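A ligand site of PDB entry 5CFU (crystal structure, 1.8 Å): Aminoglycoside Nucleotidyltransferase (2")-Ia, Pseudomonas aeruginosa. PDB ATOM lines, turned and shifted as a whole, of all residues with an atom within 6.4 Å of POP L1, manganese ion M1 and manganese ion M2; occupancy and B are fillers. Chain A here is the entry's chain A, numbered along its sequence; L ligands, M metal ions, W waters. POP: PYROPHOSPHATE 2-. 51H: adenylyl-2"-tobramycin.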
ATOM      1  N   GLY A  34      25.418 -16.311   7.046  1.00  0.00           N
ATOM      2  CA  GLY A  34      25.314 -17.009   8.322  1.00  0.00           C
ATOM      3  C   GLY A  34      25.131 -18.505   8.161  1.00  0.00           C
ATOM      4  O   GLY A  34      25.073 -19.011   7.040  1.00  0.00           O
ATOM      5  N   GLY A  35      25.057 -19.209   9.297  1.00  0.00           N
ATOM      6  CA  GLY A  35      24.720 -20.618   9.296  1.00  0.00           C
ATOM      7  C   GLY A  35      25.641 -21.435   8.419  1.00  0.00           C
ATOM      8  O   GLY A  35      26.863 -21.198   8.390  1.00  0.00           O
ATOM      9  N   GLY A  36      25.066 -22.408   7.710  1.00  0.00           N
ATOM     10  CA  GLY A  36      25.850 -23.354   6.930  1.00  0.00           C
ATOM     11  C   GLY A  36      26.707 -22.708   5.869  1.00  0.00           C
ATOM     12  O   GLY A  36      27.837 -23.135   5.643  1.00  0.00           O
ATOM     13  N   TRP A  37      26.195 -21.687   5.181  1.00  0.00           N
ATOM     14  CA  TRP A  37      27.010 -21.000   4.163  1.00  0.00           C
ATOM     15  C   TRP A  37      28.166 -20.208   4.780  1.00  0.00           C
ATOM     16  O   TRP A  37      29.209 -20.057   4.146  1.00  0.00           O
ATOM     17  CB  TRP A  37      26.155 -20.118   3.287  1.00  0.00           C
ATOM     18  CG  TRP A  37      25.604 -20.868   2.137  1.00  0.00           C
ATOM     19  CD1 TRP A  37      24.303 -21.159   1.898  1.00  0.00           C
ATOM     20  CD2 TRP A  37      26.346 -21.439   1.045  1.00  0.00           C
ATOM     21  NE1 TRP A  37      24.179 -21.880   0.737  1.00  0.00           N
ATOM     22  CE2 TRP A  37      25.425 -22.065   0.193  1.00  0.00           C
ATOM     23  CE3 TRP A  37      27.703 -21.491   0.741  1.00  0.00           C
ATOM     24  CZ2 TRP A  37      25.813 -22.735  -0.980  1.00  0.00           C
ATOM     25  CZ3 TRP A  37      28.091 -22.161  -0.432  1.00  0.00           C
ATOM     26  CH2 TRP A  37      27.152 -22.767  -1.268  1.00  0.00           C
ATOM     27  N   ILE A  39      29.801 -21.236   7.463  1.00  0.00           N
ATOM     28  CA  ILE A  39      30.794 -22.265   7.709  1.00  0.00           C
ATOM     29  C   ILE A  39      31.588 -22.523   6.424  1.00  0.00           C
ATOM     30  O   ILE A  39      32.830 -22.483   6.408  1.00  0.00           O
ATOM     31  CB  ILE A  39      30.128 -23.553   8.225  1.00  0.00           C
ATOM     32  CG1 ILE A  39      29.496 -23.281   9.591  1.00  0.00           C
ATOM     33  CG2 ILE A  39      31.141 -24.698   8.308  1.00  0.00           C
ATOM     34  CD1 ILE A  39      28.751 -24.497  10.241  1.00  0.00           C
ATOM     35  N   ARG A  48      28.497 -29.331   1.831  1.00  0.00           N
ATOM     36  CA  ARG A  48      27.259 -30.074   1.665  1.00  0.00           C
ATOM     37  C   ARG A  48      26.163 -29.189   1.100  1.00  0.00           C
ATOM     38  O   ARG A  48      26.376 -27.993   0.866  1.00  0.00           O
ATOM     39  CB  ARG A  48      26.824 -30.667   2.991  1.00  0.00           C
ATOM     40  CG  ARG A  48      26.454 -29.637   4.077  1.00  0.00           C
ATOM     41  CD  ARG A  48      25.322 -30.204   4.923  1.00  0.00           C
ATOM     42  NE  ARG A  48      25.139 -29.528   6.208  1.00  0.00           N
ATOM     43  CZ  ARG A  48      24.234 -28.585   6.463  1.00  0.00           C
ATOM     44  NH1 ARG A  48      23.410 -28.124   5.527  1.00  0.00           N
ATOM     45  NH2 ARG A  48      24.167 -28.071   7.689  1.00  0.00           N
ATOM     46  N   LYS A  49      24.986 -29.786   0.892  1.00  0.00           N
ATOM     47  CA  LYS A  49      23.803 -29.051   0.472  1.00  0.00           C
ATOM     48  C   LYS A  49      23.207 -28.246   1.641  1.00  0.00           C
ATOM     49  O   LYS A  49      23.182 -28.731   2.774  1.00  0.00           O
ATOM     50  CB  LYS A  49      22.755 -30.013  -0.085  1.00  0.00           C
ATOM     51  CG  LYS A  49      21.722 -29.357  -0.982  1.00  0.00           C
ATOM     52  CD  LYS A  49      20.566 -30.301  -1.308  1.00  0.00           C
ATOM     53  CE  LYS A  49      19.637 -30.476  -0.121  1.00  0.00           C
ATOM     54  NZ  LYS A  49      18.477 -31.355  -0.428  1.00  0.00           N
ATOM     55  N   HIS A  50      22.750 -27.036   1.359  1.00  0.00           N
ATOM     56  CA  HIS A  50      22.232 -26.105   2.357  1.00  0.00           C
ATOM     57  C   HIS A  50      20.770 -25.856   2.023  1.00  0.00           C
ATOM     58  O   HIS A  50      20.433 -25.580   0.869  1.00  0.00           O
ATOM     59  CB  HIS A  50      23.038 -24.811   2.374  1.00  0.00           C
ATOM     60  CG  HIS A  50      24.494 -25.017   2.622  1.00  0.00           C
ATOM     61  ND1 HIS A  50      24.993 -25.313   3.865  1.00  0.00           N
ATOM     62  CD2 HIS A  50      25.552 -25.049   1.773  1.00  0.00           C
ATOM     63  CE1 HIS A  50      26.295 -25.484   3.786  1.00  0.00           C
ATOM     64  NE2 HIS A  50      26.663 -25.328   2.530  1.00  0.00           N
ATOM     65  N   ASP A  51      19.905 -25.987   3.014  1.00  0.00           N
ATOM     66  CA  ASP A  51      18.459 -25.857   2.794  1.00  0.00           C
ATOM     67  C   ASP A  51      18.074 -24.427   2.503  1.00  0.00           C
ATOM     68  O   ASP A  51      17.214 -24.185   1.657  1.00  0.00           O
ATOM     69  CB  ASP A  51      17.673 -26.373   3.998  1.00  0.00           C
ATOM     70  CG  ASP A  51      17.526 -27.876   4.008  1.00  0.00           C
ATOM     71  OD1 ASP A  51      18.094 -28.531   3.104  1.00  0.00           O
ATOM     72  OD2 ASP A  51      16.839 -28.394   4.909  1.00  0.00           O
ATOM     73  N   ASP A  52      18.709 -23.478   3.174  1.00  0.00           N
ATOM     74  CA  ASP A  52      18.373 -22.064   2.990  1.00  0.00           C
ATOM     75  C   ASP A  52      19.642 -21.215   2.886  1.00  0.00           C
ATOM     76  O   ASP A  52      20.760 -21.725   2.930  1.00  0.00           O
ATOM     77  CB  ASP A  52      17.451 -21.572   4.132  1.00  0.00           C
ATOM     78  CG  ASP A  52      18.158 -21.485   5.470  1.00  0.00           C
ATOM     79  OD1 ASP A  52      19.360 -21.820   5.547  1.00  0.00           O
ATOM     80  OD2 ASP A  52      17.505 -21.096   6.464  1.00  0.00           O
ATOM     81  N   ILE A  53      19.449 -19.922   2.705  1.00  0.00           N
ATOM     82  CA  ILE A  53      20.522 -18.958   2.805  1.00  0.00           C
ATOM     83  C   ILE A  53      20.249 -18.094   4.037  1.00  0.00           C
ATOM     84  O   ILE A  53      19.211 -17.441   4.109  1.00  0.00           O
ATOM     85  CB  ILE A  53      20.620 -18.059   1.567  1.00  0.00           C
ATOM     86  CG1 ILE A  53      20.955 -18.909   0.335  1.00  0.00           C
ATOM     87  CG2 ILE A  53      21.634 -16.938   1.777  1.00  0.00           C
ATOM     88  CD1 ILE A  53      20.549 -18.267  -0.989  1.00  0.00           C
ATOM     89  N   ASP A  54      21.160 -18.118   4.993  1.00  0.00           N
ATOM     90  CA  ASP A  54      21.032 -17.347   6.212  1.00  0.00           C
ATOM     91  C   ASP A  54      21.808 -16.036   6.097  1.00  0.00           C
ATOM     92  O   ASP A  54      22.983 -16.047   5.719  1.00  0.00           O
ATOM     93  CB  ASP A  54      21.541 -18.145   7.397  1.00  0.00           C
ATOM     94  CG  ASP A  54      20.811 -19.448   7.559  1.00  0.00           C
ATOM     95  OD1 ASP A  54      19.600 -19.416   7.879  1.00  0.00           O
ATOM     96  OD2 ASP A  54      21.454 -20.495   7.325  1.00  0.00           O
ATOM     97  N   ASP A  94      16.766 -16.599   5.139  1.00  0.00           N
ATOM     98  CA  ASP A  94      16.434 -16.491   6.559  1.00  0.00           C
ATOM     99  C   ASP A  94      17.236 -15.318   7.134  1.00  0.00           C
ATOM    100  O   ASP A  94      18.454 -15.394   7.225  1.00  0.00           O
ATOM    101  CB  ASP A  94      16.767 -17.801   7.250  1.00  0.00           C
ATOM    102  CG  ASP A  94      16.174 -17.908   8.640  1.00  0.00           C
ATOM    103  OD1 ASP A  94      15.196 -18.637   8.817  1.00  0.00           O
ATOM    104  OD2 ASP A  94      16.681 -17.255   9.559  1.00  0.00           O
ATOM    105  N   TYR A 140      24.180 -22.913  17.637  1.00  0.00           N
ATOM    106  CA  TYR A 140      24.046 -24.344  17.973  1.00  0.00           C
ATOM    107  C   TYR A 140      23.741 -24.566  19.434  1.00  0.00           C
ATOM    108  O   TYR A 140      23.047 -25.525  19.795  1.00  0.00           O
ATOM    109  CB  TYR A 140      25.319 -25.129  17.592  1.00  0.00           C
ATOM    110  CG  TYR A 140      25.366 -25.489  16.129  1.00  0.00           C
ATOM    111  CD1 TYR A 140      24.548 -26.481  15.625  1.00  0.00           C
ATOM    112  CD2 TYR A 140      26.191 -24.807  15.235  1.00  0.00           C
ATOM    113  CE1 TYR A 140      24.577 -26.806  14.290  1.00  0.00           C
ATOM    114  CE2 TYR A 140      26.210 -25.134  13.897  1.00  0.00           C
ATOM    115  CZ  TYR A 140      25.412 -26.136  13.431  1.00  0.00           C
ATOM    116  OH  TYR A 140      25.422 -26.463  12.089  1.00  0.00           O
ATOM    117  N   LYS A 155      22.787 -33.784   9.647  1.00  0.00           N
ATOM    118  CA  LYS A 155      23.541 -32.741   8.944  1.00  0.00           C
ATOM    119  C   LYS A 155      23.968 -31.623   9.926  1.00  0.00           C
ATOM    120  O   LYS A 155      24.949 -30.925   9.692  1.00  0.00           O
ATOM    121  CB  LYS A 155      22.727 -32.135   7.812  1.00  0.00           C
ATOM    122  CG  LYS A 155      21.506 -31.353   8.288  1.00  0.00           C
ATOM    123  CD  LYS A 155      20.784 -30.624   7.155  1.00  0.00           C
ATOM    124  CE  LYS A 155      19.602 -29.820   7.690  1.00  0.00           C
ATOM    125  NZ  LYS A 155      18.874 -29.072   6.630  1.00  0.00           N
ATOM    126  N   HIS A 156      23.234 -31.464  11.018  1.00  0.00           N
ATOM    127  CA  HIS A 156      23.578 -30.412  11.987  1.00  0.00           C
ATOM    128  C   HIS A 156      24.515 -30.902  13.063  1.00  0.00           C
ATOM    129  O   HIS A 156      25.333 -30.138  13.557  1.00  0.00           O
ATOM    130  CB  HIS A 156      22.321 -29.817  12.597  1.00  0.00           C
ATOM    131  CG  HIS A 156      21.780 -28.716  11.754  1.00  0.00           C
ATOM    132  ND1 HIS A 156      22.566 -27.658  11.341  1.00  0.00           N
ATOM    133  CD2 HIS A 156      20.574 -28.534  11.176  1.00  0.00           C
ATOM    134  CE1 HIS A 156      21.855 -26.861  10.572  1.00  0.00           C
ATOM    135  NE2 HIS A 156      20.645 -27.370  10.455  1.00  0.00           N
ATOM    136  N   SER A 159      27.760 -30.545  11.026  1.00  0.00           N
ATOM    137  CA  SER A 159      28.187 -29.170  10.789  1.00  0.00           C
ATOM    138  C   SER A 159      28.677 -28.538  12.093  1.00  0.00           C
ATOM    139  O   SER A 159      29.643 -27.798  12.093  1.00  0.00           O
ATOM    140  CB  SER A 159      27.060 -28.351  10.155  1.00  0.00           C
ATOM    141  OG  SER A 159      26.867 -28.770   8.816  1.00  0.00           O
HETATM  142  P1  POP L   1      22.824 -24.827   7.436  1.00  0.00           P
HETATM  143  O1  POP L   1      23.973 -25.339   8.289  1.00  0.00           O
HETATM  144  O2  POP L   1      23.100 -24.881   5.943  1.00  0.00           O
HETATM  145  O3  POP L   1      22.227 -23.504   7.921  1.00  0.00           O
HETATM  146  O   POP L   1      21.686 -25.941   7.656  1.00  0.00           O
HETATM  147  P2  POP L   1      20.286 -25.937   6.846  1.00  0.00           P
HETATM  148  O4  POP L   1      19.301 -26.463   7.865  1.00  0.00           O
HETATM  149  O5  POP L   1      20.071 -24.532   6.331  1.00  0.00           O
HETATM  150  O6  POP L   1      20.533 -26.891   5.690  1.00  0.00           O
HETATM  151  O8  51H L   2      18.337 -24.284   9.607  1.00  0.00           O
HETATM  152  P   51H L   2      19.033 -22.993   9.750  1.00  0.00           P
HETATM  153  O7  51H L   2      19.651 -22.455   8.500  1.00  0.00           O
HETATM  154  O9  51H L   2      20.167 -23.093  10.827  1.00  0.00           O
HETATM  155  C14 51H L   2      21.083 -22.002  11.054  1.00  0.00           C
HETATM  156  C15 51H L   2      21.730 -22.284  12.388  1.00  0.00           C
HETATM  157  C18 51H L   2      22.386 -23.651  12.468  1.00  0.00           C
HETATM  158  O12 51H L   2      23.782 -23.525  12.203  1.00  0.00           O
HETATM  159  C17 51H L   2      22.116 -24.091  13.909  1.00  0.00           C
HETATM  160  O11 51H L   2      23.115 -23.604  14.800  1.00  0.00           O
HETATM  161  C16 51H L   2      20.786 -23.402  14.213  1.00  0.00           C
HETATM  162  N4  51H L   2      19.614 -24.209  13.945  1.00  0.00           N
HETATM  163  C21 51H L   2      18.422 -24.159  14.624  1.00  0.00           C
HETATM  164  N6  51H L   2      18.143 -23.440  15.715  1.00  0.00           N
HETATM  165  C22 51H L   2      16.879 -23.636  16.112  1.00  0.00           C
HETATM  166  N7  51H L   2      15.946 -24.409  15.553  1.00  0.00           N
HETATM  167  C23 51H L   2      16.249 -25.125  14.456  1.00  0.00           C
HETATM  168  N8  51H L   2      15.302 -25.877  13.900  1.00  0.00           N
HETATM  169  C20 51H L   2      17.561 -25.009  13.951  1.00  0.00           C
HETATM  170  N5  51H L   2      18.194 -25.598  12.873  1.00  0.00           N
HETATM  171  C19 51H L   2      19.410 -25.094  12.916  1.00  0.00           C
HETATM  172  O10 51H L   2      20.718 -22.251  13.404  1.00  0.00           O
HETATM  173  O6  51H L   2      18.057 -21.881  10.321  1.00  0.00           O
HETATM  174  C13 51H L   2      17.013 -22.249  11.239  1.00  0.00           C
HETATM  175  C12 51H L   2      15.667 -21.964  10.599  1.00  0.00           C
HETATM  176  N3  51H L   2      15.559 -22.672   9.300  1.00  0.00           N
HETATM  177  C11 51H L   2      14.546 -22.345  11.557  1.00  0.00           C
HETATM  178  O5  51H L   2      13.282 -22.055  10.985  1.00  0.00           O
HETATM  179  C9  51H L   2      14.753 -21.543  12.844  1.00  0.00           C
HETATM  180  C10 51H L   2      13.733 -21.849  13.912  1.00  0.00           C
HETATM  181  O4  51H L   2      13.773 -20.861  14.915  1.00  0.00           O
HETATM  182  O3  51H L   2      16.036 -21.830  13.423  1.00  0.00           O
HETATM  183  C8  51H L   2      17.139 -21.537  12.574  1.00  0.00           C
HETATM  184  O2  51H L   2      17.225 -20.169  12.335  1.00  0.00           O
HETATM  185  C7  51H L   2      18.184 -19.424  13.099  1.00  0.00           C
HETATM  186  C6  51H L   2      18.533 -18.173  12.288  1.00  0.00           C
HETATM  187  N2  51H L   2      18.983 -18.542  10.927  1.00  0.00           N
HETATM  188  C5  51H L   2      19.589 -17.383  13.034  1.00  0.00           C
HETATM  189  C4  51H L   2      19.124 -16.990  14.457  1.00  0.00           C
HETATM  190  N1  51H L   2      20.227 -16.360  15.187  1.00  0.00           N
HETATM  191  C24 51H L   2      17.628 -19.037  14.452  1.00  0.00           C
HETATM  192  O13 51H L   2      17.297 -20.189  15.236  1.00  0.00           O
HETATM  193  C3  51H L   2      18.663 -18.234  15.220  1.00  0.00           C
HETATM  194  O1  51H L   2      18.078 -17.787  16.455  1.00  0.00           O
HETATM  195  C2  51H L   2      18.829 -17.927  17.627  1.00  0.00           C
HETATM  196  O   51H L   2      19.344 -16.679  18.051  1.00  0.00           O
HETATM  197  C25 51H L   2      17.942 -18.560  18.707  1.00  0.00           C
HETATM  198  N9  51H L   2      17.358 -19.830  18.274  1.00  0.00           N
HETATM  199  C26 51H L   2      16.851 -17.537  19.065  1.00  0.00           C
HETATM  200  C27 51H L   2      17.421 -16.206  19.484  1.00  0.00           C
HETATM  201  O14 51H L   2      16.381 -15.237  19.689  1.00  0.00           O
HETATM  202  C1  51H L   2      18.377 -15.671  18.424  1.00  0.00           C
HETATM  203  C   51H L   2      19.150 -14.470  18.921  1.00  0.00           C
HETATM  204  N   51H L   2      20.246 -13.964  18.078  1.00  0.00           N
HETATM  205  P1  POP L   3      14.517 -26.066   9.782  1.00  0.00           P
HETATM  206  O1  POP L   3      14.552 -26.620  11.187  1.00  0.00           O
HETATM  207  O2  POP L   3      13.247 -25.297   9.473  1.00  0.00           O
HETATM  208  O3  POP L   3      15.764 -25.299   9.439  1.00  0.00           O
HETATM  209  O   POP L   3      14.440 -27.414   8.888  1.00  0.00           O
HETATM  210  P2  POP L   3      15.225 -27.785   7.520  1.00  0.00           P
HETATM  211  O4  POP L   3      15.042 -29.279   7.389  1.00  0.00           O
HETATM  212  O5  POP L   3      14.540 -26.984   6.437  1.00  0.00           O
HETATM  213  O6  POP L   3      16.671 -27.437   7.750  1.00  0.00           O
HETATM  214 MN    MN M   1      20.752 -22.549   6.840  1.00  0.00          MN
HETATM  215 MN    MN M   2      17.772 -25.812   8.676  1.00  0.00          MN
HETATM  216  O   HOH W   1      26.221 -26.810   7.309  1.00  0.00           O
HETATM  217  O   HOH W   2      17.392 -24.404   7.040  1.00  0.00           O
HETATM  218  O   HOH W   3      25.153 -24.424  10.340  1.00  0.00           O
HETATM  219  O   HOH W   4      17.755 -27.125  10.550  1.00  0.00           O
HETATM  220  O   HOH W   5      22.125 -22.478   5.109  1.00  0.00           O
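Manganese ion M1 is bound by an oxygen (O7) of 51H L2, the side-chain carboxylate (OD1) of Asp 52, an oxygen (O3) of POP L1, an oxygen (O5) of POP L1, water W5 and the side-chain carboxylate (OD2) of Asp 54. Manganese ion M1 has six donor atoms within binding distance.
The nearest printed residue that does not touch manganese ion M1 is Gly 36 (4.4 Å).
Hydrophobic or aromatic side chains that line POP L1: His 50 and His 156. Within 4 Å of POP L1: Gly 36, Arg 48, His 50, Asp 51, Asp 52, Asp 54, Lys 155 and His 156.
Water W5 lies within hydrogen-bond range of the backbone carbonyl oxygen (O) of Asp 52 (2.7 Å) and an oxygen (O2) of POP L1 (2.7 Å). Water W4 lies within hydrogen-bond range of N5 of 51H L2 (2.8 Å), NE2 of His 156 (2.9 Å) and O1 of POP L3 (3.3 Å). Water W2 bridges OD2 of Asp 52 (3.4 Å) and N3 of 51H L2 (3.4 Å). Water W3 lies within hydrogen-bond range of an oxygen (O12) of 51H L2, an oxygen (O1) of POP L1, the side-chain hydroxyl (OH) of Tyr 140 and the backbone NH (N) of Gly 36. Water W1 lies within hydrogen-bond range of NH2 of Arg 48, OG of Ser 159 and O1 of POP L1.
NE2 of His 156 touches manganese ion M2, at 3.7 Å. Of the 17 residues printed, 1 comes within 4 Å of manganese ion M2. The nearest printed residue that does not touch manganese ion M2 is Lys 155 (4.004 Å).
An oxygen (O1) of POP L1 lies within salt-bridge range of the guanidinium group (NH2) of Arg 48 (2.8 Å). A ring nitrogen (ND1) of His 50 sits at hydrogen-bond distance from an oxygen (O2) of POP L1. An oxygen (O6) of POP L1 is in hydrogen-bond range of the backbone NH (N) of Asp 51, 2.9 Å away. O6 of POP L1 lies within salt-bridge range of NZ of Lys 155 (2.9 Å). N of Gly 36 sits close to O1 of POP L1 (3.2 Å). A ring nitrogen (NE2) of His 156 sits close to an oxygen (O) of POP L1. N of Tyr 140 is in hydrogen-bond range of O11 of 51H L2 (3.1 Å). OH of Tyr 140 lies close to O12 of 51H L2, at 3.4 Å. A nitrogen (N2) of 51H L2 is in salt-bridge range of the side-chain carboxylate (OD2) of Asp 94 (3.0 Å). An oxygen (O5) of POP L3 sits close to the side-chain carboxylate of Asp 51. NZ of Lys 155 is in salt-bridge range of O4 of POP L3 (3.9 Å).
Manganese ion M2 is bound by O4 of POP L1 (1.8 Å), O8 of 51H L2 (1.9 Å), O6 of POP L3 (2.2 Å), water W2 (2.2 Å), O3 of POP L3 (2.2 Å) and water W4 (2.3 Å).
The backbone carbonyl oxygen of Asp 54 is in hydrogen-bond range of the backbone NH of Gly 34, at 2.8 Å. A ring nitrogen (NE2) of His 50 sits at hydrogen-bond distance from the backbone carbonyl oxygen (O) of Arg 48, at 3.2 Å. The side-chain hydroxyl (OG) of Ser 159 sits at hydrogen-bond distance from the guanidinium group (NH2) of Arg 48. The side-chain carboxylate of Asp 51 is in salt-bridge range of the side-chain amino group of Lys 155 (2.8 Å). O of Lys 155 is in hydrogen-bond range of OG of Ser 159 (3.0 Å). OH of Tyr 140 sits at hydrogen-bond distance from ND1 of His 156.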
